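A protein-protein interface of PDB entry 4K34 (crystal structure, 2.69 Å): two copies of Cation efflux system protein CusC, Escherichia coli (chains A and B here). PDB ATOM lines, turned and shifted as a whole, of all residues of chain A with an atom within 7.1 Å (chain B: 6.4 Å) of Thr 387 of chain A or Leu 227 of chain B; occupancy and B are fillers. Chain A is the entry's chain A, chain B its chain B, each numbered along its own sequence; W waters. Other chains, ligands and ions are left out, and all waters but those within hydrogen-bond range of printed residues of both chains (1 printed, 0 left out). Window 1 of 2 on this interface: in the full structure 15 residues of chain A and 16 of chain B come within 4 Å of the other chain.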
ATOM      1  N   ARG A 379       8.954  -1.604 -11.716  1.00  0.00           N
ATOM      2  CA  ARG A 379       7.543  -1.525 -11.394  1.00  0.00           C
ATOM      3  C   ARG A 379       7.329  -1.010  -9.954  1.00  0.00           C
ATOM      4  O   ARG A 379       6.489  -0.127  -9.706  1.00  0.00           O
ATOM      5  CB  ARG A 379       6.909  -2.905 -11.591  1.00  0.00           C
ATOM      6  CG  ARG A 379       5.476  -3.044 -11.133  1.00  0.00           C
ATOM      7  CD  ARG A 379       5.062  -4.509 -11.102  1.00  0.00           C
ATOM      8  NE  ARG A 379       4.291  -4.916 -12.286  1.00  0.00           N
ATOM      9  CZ  ARG A 379       4.789  -5.634 -13.292  1.00  0.00           C
ATOM     10  NH1 ARG A 379       6.063  -6.025 -13.263  1.00  0.00           N
ATOM     11  NH2 ARG A 379       4.021  -5.962 -14.327  1.00  0.00           N
ATOM     12  N   TYR A 380       8.084  -1.564  -9.006  1.00  0.00           N
ATOM     13  CA  TYR A 380       7.984  -1.098  -7.634  1.00  0.00           C
ATOM     14  C   TYR A 380       8.293   0.395  -7.625  1.00  0.00           C
ATOM     15  O   TYR A 380       7.562   1.165  -7.017  1.00  0.00           O
ATOM     16  CB  TYR A 380       8.904  -1.870  -6.675  1.00  0.00           C
ATOM     17  CG  TYR A 380       8.825  -3.404  -6.782  1.00  0.00           C
ATOM     18  CD1 TYR A 380       7.635  -4.067  -7.203  1.00  0.00           C
ATOM     19  CD2 TYR A 380       9.948  -4.200  -6.455  1.00  0.00           C
ATOM     20  CE1 TYR A 380       7.580  -5.471  -7.306  1.00  0.00           C
ATOM     21  CE2 TYR A 380       9.898  -5.598  -6.545  1.00  0.00           C
ATOM     22  CZ  TYR A 380       8.723  -6.224  -6.974  1.00  0.00           C
ATOM     23  OH  TYR A 380       8.728  -7.594  -7.065  1.00  0.00           O
ATOM     24  N   LEU A 381       9.338   0.799  -8.352  1.00  0.00           N
ATOM     25  CA  LEU A 381       9.779   2.195  -8.388  1.00  0.00           C
ATOM     26  C   LEU A 381       8.740   3.184  -8.947  1.00  0.00           C
ATOM     27  O   LEU A 381       8.554   4.284  -8.417  1.00  0.00           O
ATOM     28  CB  LEU A 381      11.073   2.322  -9.189  1.00  0.00           C
ATOM     29  CG  LEU A 381      11.622   3.752  -9.222  1.00  0.00           C
ATOM     30  CD1 LEU A 381      12.485   4.067  -7.992  1.00  0.00           C
ATOM     31  CD2 LEU A 381      12.364   4.010 -10.497  1.00  0.00           C
ATOM     32  N   ALA A 382       8.081   2.788 -10.031  1.00  0.00           N
ATOM     33  CA  ALA A 382       7.074   3.624 -10.659  1.00  0.00           C
ATOM     34  C   ALA A 382       5.926   3.907  -9.680  1.00  0.00           C
ATOM     35  O   ALA A 382       5.471   5.050  -9.576  1.00  0.00           O
ATOM     36  CB  ALA A 382       6.573   2.979 -11.945  1.00  0.00           C
ATOM     37  N   SER A 383       5.494   2.876  -8.949  1.00  0.00           N
ATOM     38  CA  SER A 383       4.514   3.031  -7.872  1.00  0.00           C
ATOM     39  C   SER A 383       5.004   3.888  -6.697  1.00  0.00           C
ATOM     40  O   SER A 383       4.237   4.653  -6.127  1.00  0.00           O
ATOM     41  CB  SER A 383       4.061   1.669  -7.336  1.00  0.00           C
ATOM     42  OG  SER A 383       3.267   0.988  -8.284  1.00  0.00           O
ATOM     43  N   LEU A 384       6.263   3.734  -6.311  1.00  0.00           N
ATOM     44  CA  LEU A 384       6.839   4.585  -5.276  1.00  0.00           C
ATOM     45  C   LEU A 384       6.885   6.046  -5.768  1.00  0.00           C
ATOM     46  O   LEU A 384       6.564   6.959  -5.017  1.00  0.00           O
ATOM     47  CB  LEU A 384       8.222   4.074  -4.825  1.00  0.00           C
ATOM     48  CG  LEU A 384       8.283   2.773  -3.998  1.00  0.00           C
ATOM     49  CD1 LEU A 384       9.705   2.225  -3.850  1.00  0.00           C
ATOM     50  CD2 LEU A 384       7.688   2.963  -2.630  1.00  0.00           C
ATOM     51  N   GLN A 385       7.251   6.258  -7.032  1.00  0.00           N
ATOM     52  CA  GLN A 385       7.255   7.609  -7.601  1.00  0.00           C
ATOM     53  C   GLN A 385       5.876   8.273  -7.579  1.00  0.00           C
ATOM     54  O   GLN A 385       5.751   9.428  -7.162  1.00  0.00           O
ATOM     55  CB  GLN A 385       7.803   7.618  -9.026  1.00  0.00           C
ATOM     56  CG  GLN A 385       9.257   7.261  -9.107  1.00  0.00           C
ATOM     57  CD  GLN A 385       9.785   7.247 -10.536  1.00  0.00           C
ATOM     58  OE1 GLN A 385       9.288   6.510 -11.407  1.00  0.00           O
ATOM     59  NE2 GLN A 385      10.801   8.064 -10.785  1.00  0.00           N
ATOM     60  N   ILE A 386       4.851   7.552  -8.028  1.00  0.00           N
ATOM     61  CA  ILE A 386       3.499   8.092  -8.005  1.00  0.00           C
ATOM     62  C   ILE A 386       3.076   8.397  -6.556  1.00  0.00           C
ATOM     63  O   ILE A 386       2.563   9.475  -6.260  1.00  0.00           O
ATOM     64  CB  ILE A 386       2.467   7.176  -8.773  1.00  0.00           C
ATOM     65  CG1 ILE A 386       1.163   7.918  -9.040  1.00  0.00           C
ATOM     66  CG2 ILE A 386       2.166   5.879  -8.042  1.00  0.00           C
ATOM     67  CD1 ILE A 386       1.006   8.349 -10.475  1.00  0.00           C
ATOM     68  N   THR A 387       3.357   7.468  -5.654  1.00  0.00           N
ATOM     69  CA  THR A 387       3.026   7.616  -4.253  1.00  0.00           C
ATOM     70  C   THR A 387       3.721   8.813  -3.608  1.00  0.00           C
ATOM     71  O   THR A 387       3.177   9.432  -2.700  1.00  0.00           O
ATOM     72  CB  THR A 387       3.358   6.316  -3.489  1.00  0.00           C
ATOM     73  OG1 THR A 387       2.533   5.262  -3.991  1.00  0.00           O
ATOM     74  CG2 THR A 387       3.095   6.463  -2.008  1.00  0.00           C
ATOM     75  N   LEU A 388       4.908   9.165  -4.091  1.00  0.00           N
ATOM     76  CA  LEU A 388       5.604  10.318  -3.539  1.00  0.00           C
ATOM     77  C   LEU A 388       4.995  11.629  -4.010  1.00  0.00           C
ATOM     78  O   LEU A 388       4.786  12.528  -3.209  1.00  0.00           O
ATOM     79  CB  LEU A 388       7.097  10.284  -3.847  1.00  0.00           C
ATOM     80  CG  LEU A 388       7.891  11.484  -3.313  1.00  0.00           C
ATOM     81  CD1 LEU A 388       7.701  11.636  -1.824  1.00  0.00           C
ATOM     82  CD2 LEU A 388       9.334  11.282  -3.626  1.00  0.00           C
ATOM     83  N   GLN A 389       4.712  11.726  -5.301  1.00  0.00           N
ATOM     84  CA  GLN A 389       4.059  12.906  -5.858  1.00  0.00           C
ATOM     85  C   GLN A 389       2.754  13.161  -5.124  1.00  0.00           C
ATOM     86  O   GLN A 389       2.465  14.286  -4.722  1.00  0.00           O
ATOM     87  CB  GLN A 389       3.752  12.694  -7.338  1.00  0.00           C
ATOM     88  CG  GLN A 389       4.953  12.331  -8.187  1.00  0.00           C
ATOM     89  CD  GLN A 389       4.547  11.736  -9.540  1.00  0.00           C
ATOM     90  OE1 GLN A 389       3.468  12.032 -10.063  1.00  0.00           O
ATOM     91  NE2 GLN A 389       5.410  10.884 -10.103  1.00  0.00           N
ATOM     92  N   ARG A 390       1.975  12.101  -4.936  1.00  0.00           N
ATOM     93  CA  ARG A 390       0.684  12.227  -4.297  1.00  0.00           C
ATOM     94  C   ARG A 390       0.828  12.663  -2.844  1.00  0.00           C
ATOM     95  O   ARG A 390       0.096  13.548  -2.369  1.00  0.00           O
ATOM     96  CB  ARG A 390      -0.104  10.934  -4.454  1.00  0.00           C
ATOM     97  CG  ARG A 390      -0.350  10.608  -5.928  1.00  0.00           C
ATOM     98  CD  ARG A 390      -1.651   9.892  -6.179  1.00  0.00           C
ATOM     99  NE  ARG A 390      -1.560   8.465  -5.907  1.00  0.00           N
ATOM    100  CZ  ARG A 390      -1.820   7.506  -6.795  1.00  0.00           C
ATOM    101  NH1 ARG A 390      -2.202   7.818  -8.032  1.00  0.00           N
ATOM    102  NH2 ARG A 390      -1.707   6.227  -6.436  1.00  0.00           N
ATOM    103  N   ALA A 391       1.806  12.078  -2.158  1.00  0.00           N
ATOM    104  CA  ALA A 391       2.106  12.464  -0.784  1.00  0.00           C
ATOM    105  C   ALA A 391       2.522  13.941  -0.679  1.00  0.00           C
ATOM    106  O   ALA A 391       2.146  14.623   0.266  1.00  0.00           O
ATOM    107  CB  ALA A 391       3.169  11.560  -0.199  1.00  0.00           C
ATOM    108  N   ARG A 392       3.290  14.433  -1.650  1.00  0.00           N
ATOM    109  CA  ARG A 392       3.706  15.836  -1.654  1.00  0.00           C
ATOM    110  C   ARG A 392       2.540  16.804  -1.833  1.00  0.00           C
ATOM    111  O   ARG A 392       2.441  17.818  -1.131  1.00  0.00           O
ATOM    112  CB  ARG A 392       4.739  16.086  -2.739  1.00  0.00           C
ATOM    113  CG  ARG A 392       6.085  15.578  -2.377  1.00  0.00           C
ATOM    114  CD  ARG A 392       7.075  15.733  -3.500  1.00  0.00           C
ATOM    115  NE  ARG A 392       8.411  15.605  -2.935  1.00  0.00           N
ATOM    116  CZ  ARG A 392       9.467  15.119  -3.576  1.00  0.00           C
ATOM    117  NH1 ARG A 392       9.358  14.706  -4.835  1.00  0.00           N
ATOM    118  NH2 ARG A 392      10.636  15.045  -2.947  1.00  0.00           N
ATOM    119  N   ALA A 408       8.426   8.330   2.616  1.00  0.00           N
ATOM    120  CA  ALA A 408       8.130   7.884   1.269  1.00  0.00           C
ATOM    121  C   ALA A 408       9.341   8.047   0.350  1.00  0.00           C
ATOM    122  O   ALA A 408       9.614   7.190  -0.492  1.00  0.00           O
ATOM    123  CB  ALA A 408       6.919   8.628   0.715  1.00  0.00           C
ATOM    124  N   ASN B  57       1.947   1.629   9.341  1.00  0.00           N
ATOM    125  CA  ASN B  57       0.902   2.492   8.822  1.00  0.00           C
ATOM    126  C   ASN B  57       0.184   3.261   9.907  1.00  0.00           C
ATOM    127  O   ASN B  57      -1.040   3.191  10.056  1.00  0.00           O
ATOM    128  CB  ASN B  57      -0.030   1.738   7.869  1.00  0.00           C
ATOM    129  CG  ASN B  57       0.650   1.412   6.542  1.00  0.00           C
ATOM    130  OD1 ASN B  57       0.664   2.239   5.633  1.00  0.00           O
ATOM    131  ND2 ASN B  57       1.241   0.218   6.437  1.00  0.00           N
ATOM    132  N   MET B  62      -1.950   8.407   4.515  1.00  0.00           N
ATOM    133  CA  MET B  62      -0.934   7.597   3.846  1.00  0.00           C
ATOM    134  C   MET B  62      -1.361   6.138   3.551  1.00  0.00           C
ATOM    135  O   MET B  62      -1.099   5.620   2.456  1.00  0.00           O
ATOM    136  CB  MET B  62       0.374   7.605   4.645  1.00  0.00           C
ATOM    137  CG  MET B  62       1.123   8.929   4.610  1.00  0.00           C
ATOM    138  SD  MET B  62       1.415   9.539   2.927  1.00  0.00           S
ATOM    139  CE  MET B  62       2.491   8.246   2.270  1.00  0.00           C
ATOM    140  N   LEU B  65      -3.338   5.992   0.642  1.00  0.00           N
ATOM    141  CA  LEU B  65      -2.529   6.111  -0.575  1.00  0.00           C
ATOM    142  C   LEU B  65      -1.968   4.775  -1.021  1.00  0.00           C
ATOM    143  O   LEU B  65      -1.980   4.427  -2.210  1.00  0.00           O
ATOM    144  CB  LEU B  65      -1.340   7.046  -0.343  1.00  0.00           C
ATOM    145  CG  LEU B  65      -1.573   8.521  -0.584  1.00  0.00           C
ATOM    146  CD1 LEU B  65      -0.295   9.125  -1.118  1.00  0.00           C
ATOM    147  CD2 LEU B  65      -2.731   8.690  -1.556  1.00  0.00           C
ATOM    148  N   LYS B  66      -1.422   4.060  -0.049  1.00  0.00           N
ATOM    149  CA  LYS B  66      -0.767   2.803  -0.304  1.00  0.00           C
ATOM    150  C   LYS B  66      -1.771   1.802  -0.853  1.00  0.00           C
ATOM    151  O   LYS B  66      -1.479   1.101  -1.826  1.00  0.00           O
ATOM    152  CB  LYS B  66      -0.090   2.311   0.977  1.00  0.00           C
ATOM    153  CG  LYS B  66       1.025   3.259   1.432  1.00  0.00           C
ATOM    154  CD  LYS B  66       1.606   2.932   2.817  1.00  0.00           C
ATOM    155  CE  LYS B  66       2.680   3.990   3.209  1.00  0.00           C
ATOM    156  NZ  LYS B  66       3.288   3.858   4.589  1.00  0.00           N
ATOM    157  N   VAL B  67      -2.962   1.768  -0.257  1.00  0.00           N
ATOM    158  CA  VAL B  67      -3.976   0.829  -0.688  1.00  0.00           C
ATOM    159  C   VAL B  67      -4.427   1.215  -2.080  1.00  0.00           C
ATOM    160  O   VAL B  67      -4.692   0.366  -2.922  1.00  0.00           O
ATOM    161  CB  VAL B  67      -5.191   0.778   0.287  1.00  0.00           C
ATOM    162  CG1 VAL B  67      -6.272  -0.179  -0.223  1.00  0.00           C
ATOM    163  CG2 VAL B  67      -4.749   0.363   1.674  1.00  0.00           C
ATOM    164  N   GLU B  69      -2.741   2.616  -4.472  1.00  0.00           N
ATOM    165  CA  GLU B  69      -1.739   2.300  -5.487  1.00  0.00           C
ATOM    166  C   GLU B  69      -1.549   0.802  -5.683  1.00  0.00           C
ATOM    167  O   GLU B  69      -1.370   0.341  -6.812  1.00  0.00           O
ATOM    168  CB  GLU B  69      -0.408   2.958  -5.157  1.00  0.00           C
ATOM    169  CG  GLU B  69       0.690   2.697  -6.182  1.00  0.00           C
ATOM    170  CD  GLU B  69       0.273   3.024  -7.607  1.00  0.00           C
ATOM    171  OE1 GLU B  69      -0.608   3.896  -7.798  1.00  0.00           O
ATOM    172  OE2 GLU B  69       0.827   2.406  -8.545  1.00  0.00           O
ATOM    173  N   ALA B  70      -1.590   0.053  -4.582  1.00  0.00           N
ATOM    174  CA  ALA B  70      -1.668  -1.410  -4.629  1.00  0.00           C
ATOM    175  C   ALA B  70      -2.837  -1.999  -5.468  1.00  0.00           C
ATOM    176  O   ALA B  70      -2.765  -3.129  -5.935  1.00  0.00           O
ATOM    177  CB  ALA B  70      -1.710  -1.964  -3.223  1.00  0.00           C
ATOM    178  N   GLN B  73      -2.603  -0.495  -9.654  1.00  0.00           N
ATOM    179  CA  GLN B  73      -1.527  -1.006 -10.478  1.00  0.00           C
ATOM    180  C   GLN B  73      -1.989  -2.209 -11.307  1.00  0.00           C
ATOM    181  O   GLN B  73      -1.344  -2.590 -12.287  1.00  0.00           O
ATOM    182  CB  GLN B  73      -0.253  -1.220  -9.627  1.00  0.00           C
ATOM    183  CG  GLN B  73       0.472  -2.523  -9.752  1.00  0.00           C
ATOM    184  CD  GLN B  73       0.134  -3.449  -8.624  1.00  0.00           C
ATOM    185  OE1 GLN B  73      -0.989  -3.460  -8.126  1.00  0.00           O
ATOM    186  NE2 GLN B  73       1.101  -4.230  -8.208  1.00  0.00           N
ATOM    187  N   ASN B 222       3.662  -8.771  -5.531  1.00  0.00           N
ATOM    188  CA  ASN B 222       4.849  -8.309  -4.806  1.00  0.00           C
ATOM    189  C   ASN B 222       4.884  -6.801  -4.650  1.00  0.00           C
ATOM    190  O   ASN B 222       5.222  -6.290  -3.594  1.00  0.00           O
ATOM    191  CB  ASN B 222       6.132  -8.776  -5.484  1.00  0.00           C
ATOM    192  CG  ASN B 222       6.504 -10.193  -5.115  1.00  0.00           C
ATOM    193  OD1 ASN B 222       6.138 -10.693  -4.049  1.00  0.00           O
ATOM    194  ND2 ASN B 222       7.235 -10.853  -5.996  1.00  0.00           N
ATOM    195  N   ASN B 223       4.517  -6.104  -5.711  1.00  0.00           N
ATOM    196  CA  ASN B 223       4.388  -4.658  -5.700  1.00  0.00           C
ATOM    197  C   ASN B 223       3.395  -4.234  -4.629  1.00  0.00           C
ATOM    198  O   ASN B 223       3.699  -3.395  -3.776  1.00  0.00           O
ATOM    199  CB  ASN B 223       3.945  -4.187  -7.089  1.00  0.00           C
ATOM    200  CG  ASN B 223       4.047  -2.675  -7.283  1.00  0.00           C
ATOM    201  OD1 ASN B 223       4.697  -1.961  -6.518  1.00  0.00           O
ATOM    202  ND2 ASN B 223       3.402  -2.185  -8.339  1.00  0.00           N
ATOM    203  N   ALA B 224       2.223  -4.855  -4.647  1.00  0.00           N
ATOM    204  CA  ALA B 224       1.193  -4.582  -3.652  1.00  0.00           C
ATOM    205  C   ALA B 224       1.688  -4.809  -2.228  1.00  0.00           C
ATOM    206  O   ALA B 224       1.502  -3.953  -1.361  1.00  0.00           O
ATOM    207  CB  ALA B 224      -0.017  -5.404  -3.928  1.00  0.00           C
ATOM    208  N   LEU B 225       2.349  -5.938  -1.988  1.00  0.00           N
ATOM    209  CA  LEU B 225       2.878  -6.227  -0.654  1.00  0.00           C
ATOM    210  C   LEU B 225       3.945  -5.263  -0.153  1.00  0.00           C
ATOM    211  O   LEU B 225       3.895  -4.876   1.008  1.00  0.00           O
ATOM    212  CB  LEU B 225       3.378  -7.666  -0.538  1.00  0.00           C
ATOM    213  CG  LEU B 225       2.324  -8.732  -0.252  1.00  0.00           C
ATOM    214  CD1 LEU B 225       2.945 -10.115  -0.312  1.00  0.00           C
ATOM    215  CD2 LEU B 225       1.681  -8.505   1.102  1.00  0.00           C
ATOM    216  N   GLN B 226       4.910  -4.886  -1.001  1.00  0.00           N
ATOM    217  CA  GLN B 226       5.943  -3.902  -0.614  1.00  0.00           C
ATOM    218  C   GLN B 226       5.299  -2.574  -0.257  1.00  0.00           C
ATOM    219  O   GLN B 226       5.667  -1.919   0.719  1.00  0.00           O
ATOM    220  CB  GLN B 226       6.922  -3.625  -1.751  1.00  0.00           C
ATOM    221  CG  GLN B 226       7.503  -4.819  -2.440  1.00  0.00           C
ATOM    222  CD  GLN B 226       8.917  -5.089  -2.035  1.00  0.00           C
ATOM    223  OE1 GLN B 226       9.207  -5.295  -0.853  1.00  0.00           O
ATOM    224  NE2 GLN B 226       9.821  -5.093  -3.013  1.00  0.00           N
ATOM    225  N   LEU B 227       4.343  -2.173  -1.082  1.00  0.00           N
ATOM    226  CA  LEU B 227       3.620  -0.930  -0.863  1.00  0.00           C
ATOM    227  C   LEU B 227       2.872  -0.890   0.458  1.00  0.00           C
ATOM    228  O   LEU B 227       2.996   0.059   1.202  1.00  0.00           O
ATOM    229  CB  LEU B 227       2.620  -0.700  -1.995  1.00  0.00           C
ATOM    230  CG  LEU B 227       3.197  -0.021  -3.221  1.00  0.00           C
ATOM    231  CD1 LEU B 227       2.386  -0.406  -4.444  1.00  0.00           C
ATOM    232  CD2 LEU B 227       3.160   1.475  -2.976  1.00  0.00           C
ATOM    233  N   LEU B 228       2.066  -1.916   0.726  1.00  0.00           N
ATOM    234  CA  LEU B 228       1.227  -1.938   1.917  1.00  0.00           C
ATOM    235  C   LEU B 228       2.082  -1.964   3.172  1.00  0.00           C
ATOM    236  O   LEU B 228       1.700  -1.401   4.205  1.00  0.00           O
ATOM    237  CB  LEU B 228       0.285  -3.138   1.873  1.00  0.00           C
ATOM    238  CG  LEU B 228      -0.589  -2.997   0.636  1.00  0.00           C
ATOM    239  CD1 LEU B 228      -1.469  -4.221   0.392  1.00  0.00           C
ATOM    240  CD2 LEU B 228      -1.396  -1.693   0.720  1.00  0.00           C
ATOM    241  N   LEU B 229       3.240  -2.607   3.070  1.00  0.00           N
ATOM    242  CA  LEU B 229       4.199  -2.637   4.157  1.00  0.00           C
ATOM    243  C   LEU B 229       5.190  -1.474   4.057  1.00  0.00           C
ATOM    244  O   LEU B 229       4.855  -0.313   4.356  1.00  0.00           O
ATOM    245  CB  LEU B 229       4.977  -3.943   4.123  1.00  0.00           C
ATOM    246  CG  LEU B 229       4.455  -5.127   4.927  1.00  0.00           C
ATOM    247  CD1 LEU B 229       3.016  -5.432   4.584  1.00  0.00           C
ATOM    248  CD2 LEU B 229       5.330  -6.332   4.652  1.00  0.00           C
ATOM    249  N   GLY B 230       6.410  -1.800   3.629  1.00  0.00           N
ATOM    250  CA  GLY B 230       7.510  -0.853   3.619  1.00  0.00           C
ATOM    251  C   GLY B 230       8.682  -1.299   2.759  1.00  0.00           C
ATOM    252  O   GLY B 230       8.757  -2.457   2.312  1.00  0.00           O
HETATM  253  O   HOH W   1      -0.083   5.938  -4.578  1.00  0.00           O
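OE1 of Glu 69 of chain B lies within salt-bridge range of NH2 of Arg 390 of chain A (2.9 Å). ND2 of Asn 223 of chain B lies within hydrogen-bond range of OG of Ser 383 of chain A (3.2 Å). OG of Ser 383 of chain A lies within hydrogen-bond range of OE2 of Glu 69 of chain B (2.8 Å).
Asn 223 of chain B touches Arg 379 of chain A (ND2 to CG, 3.6 Å). Asn 222 of chain B touches Tyr 380 of chain A. Tyr 380 of chain A touches Asn 223 of chain B. Tyr 380 of chain A touches Gln 226 of chain B. Leu 227 of chain B touches Ser 383 of chain A. Glu 69 of chain B touches Ile 386 of chain A. O of Thr 387 of chain A touches CD1 of Leu 65 of chain B, at 3.8 Å. Thr 387 of chain A touches Glu 69 of chain B. Leu 65 of chain B touches Arg 390 of chain A. N of Ala 391 of chain A touches CD1 of Leu 65 of chain B (3.8 Å).
Hydrophobic or aromatic side chains of chain B that line the printed part of chain A: Leu 65 and Leu 227. Among the printed residues, 14 pairs touch across the chains.
Leu 227 of chain B touches just these residues of chain A: Ser 383 and Thr 387. Of the printed residues of chain B, Arg 379 of chain A touches Asn 223 (3.6 Å). Of the printed residues of chain B, Tyr 380 of chain A touches Asn 222 (3.3 Å), Asn 223 (3.5 Å) and Gln 226 (3.6 Å). Of the printed residues of chain B, Ala 391 of chain A touches Leu 65. Of the printed residues of chain B, Arg 390 of chain A touches Leu 65 (3.8 Å) and Glu 69 (2.9 Å). Of the printed residues of chain A, Asn 223 of chain B touches Arg 379, Tyr 380 and Ser 383. The nearest residue of chain B that does not touch Thr 387 of chain A is Met 62 of chain B (4.7 Å). The nearest residue of chain A that does not touch Leu 227 of chain B is Leu 384 of chain A (4.8 Å).
No position is printed for both chains. Of the 14 pairs that touch across the chains among the printed residues, none has its exchanged pair printed and touching as well.
Water W1 lies within hydrogen-bond range of NH2 of Arg 390 of chain A (2.5 Å), OG1 of Thr 387 of chain A (2.8 Å) and O of Leu 65 of chain B (3.4 Å).
The side-chain hydroxyl of Thr 387 of chain A sits at hydrogen-bond distance from the backbone carbonyl oxygen of Ser 383 of chain A, at 2.8 Å. The side-chain amide nitrogen (NE2) of Gln 73 of chain B lies close to the side-chain amide nitrogen (ND2) of Asn 223 of chain B (3.1 Å).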
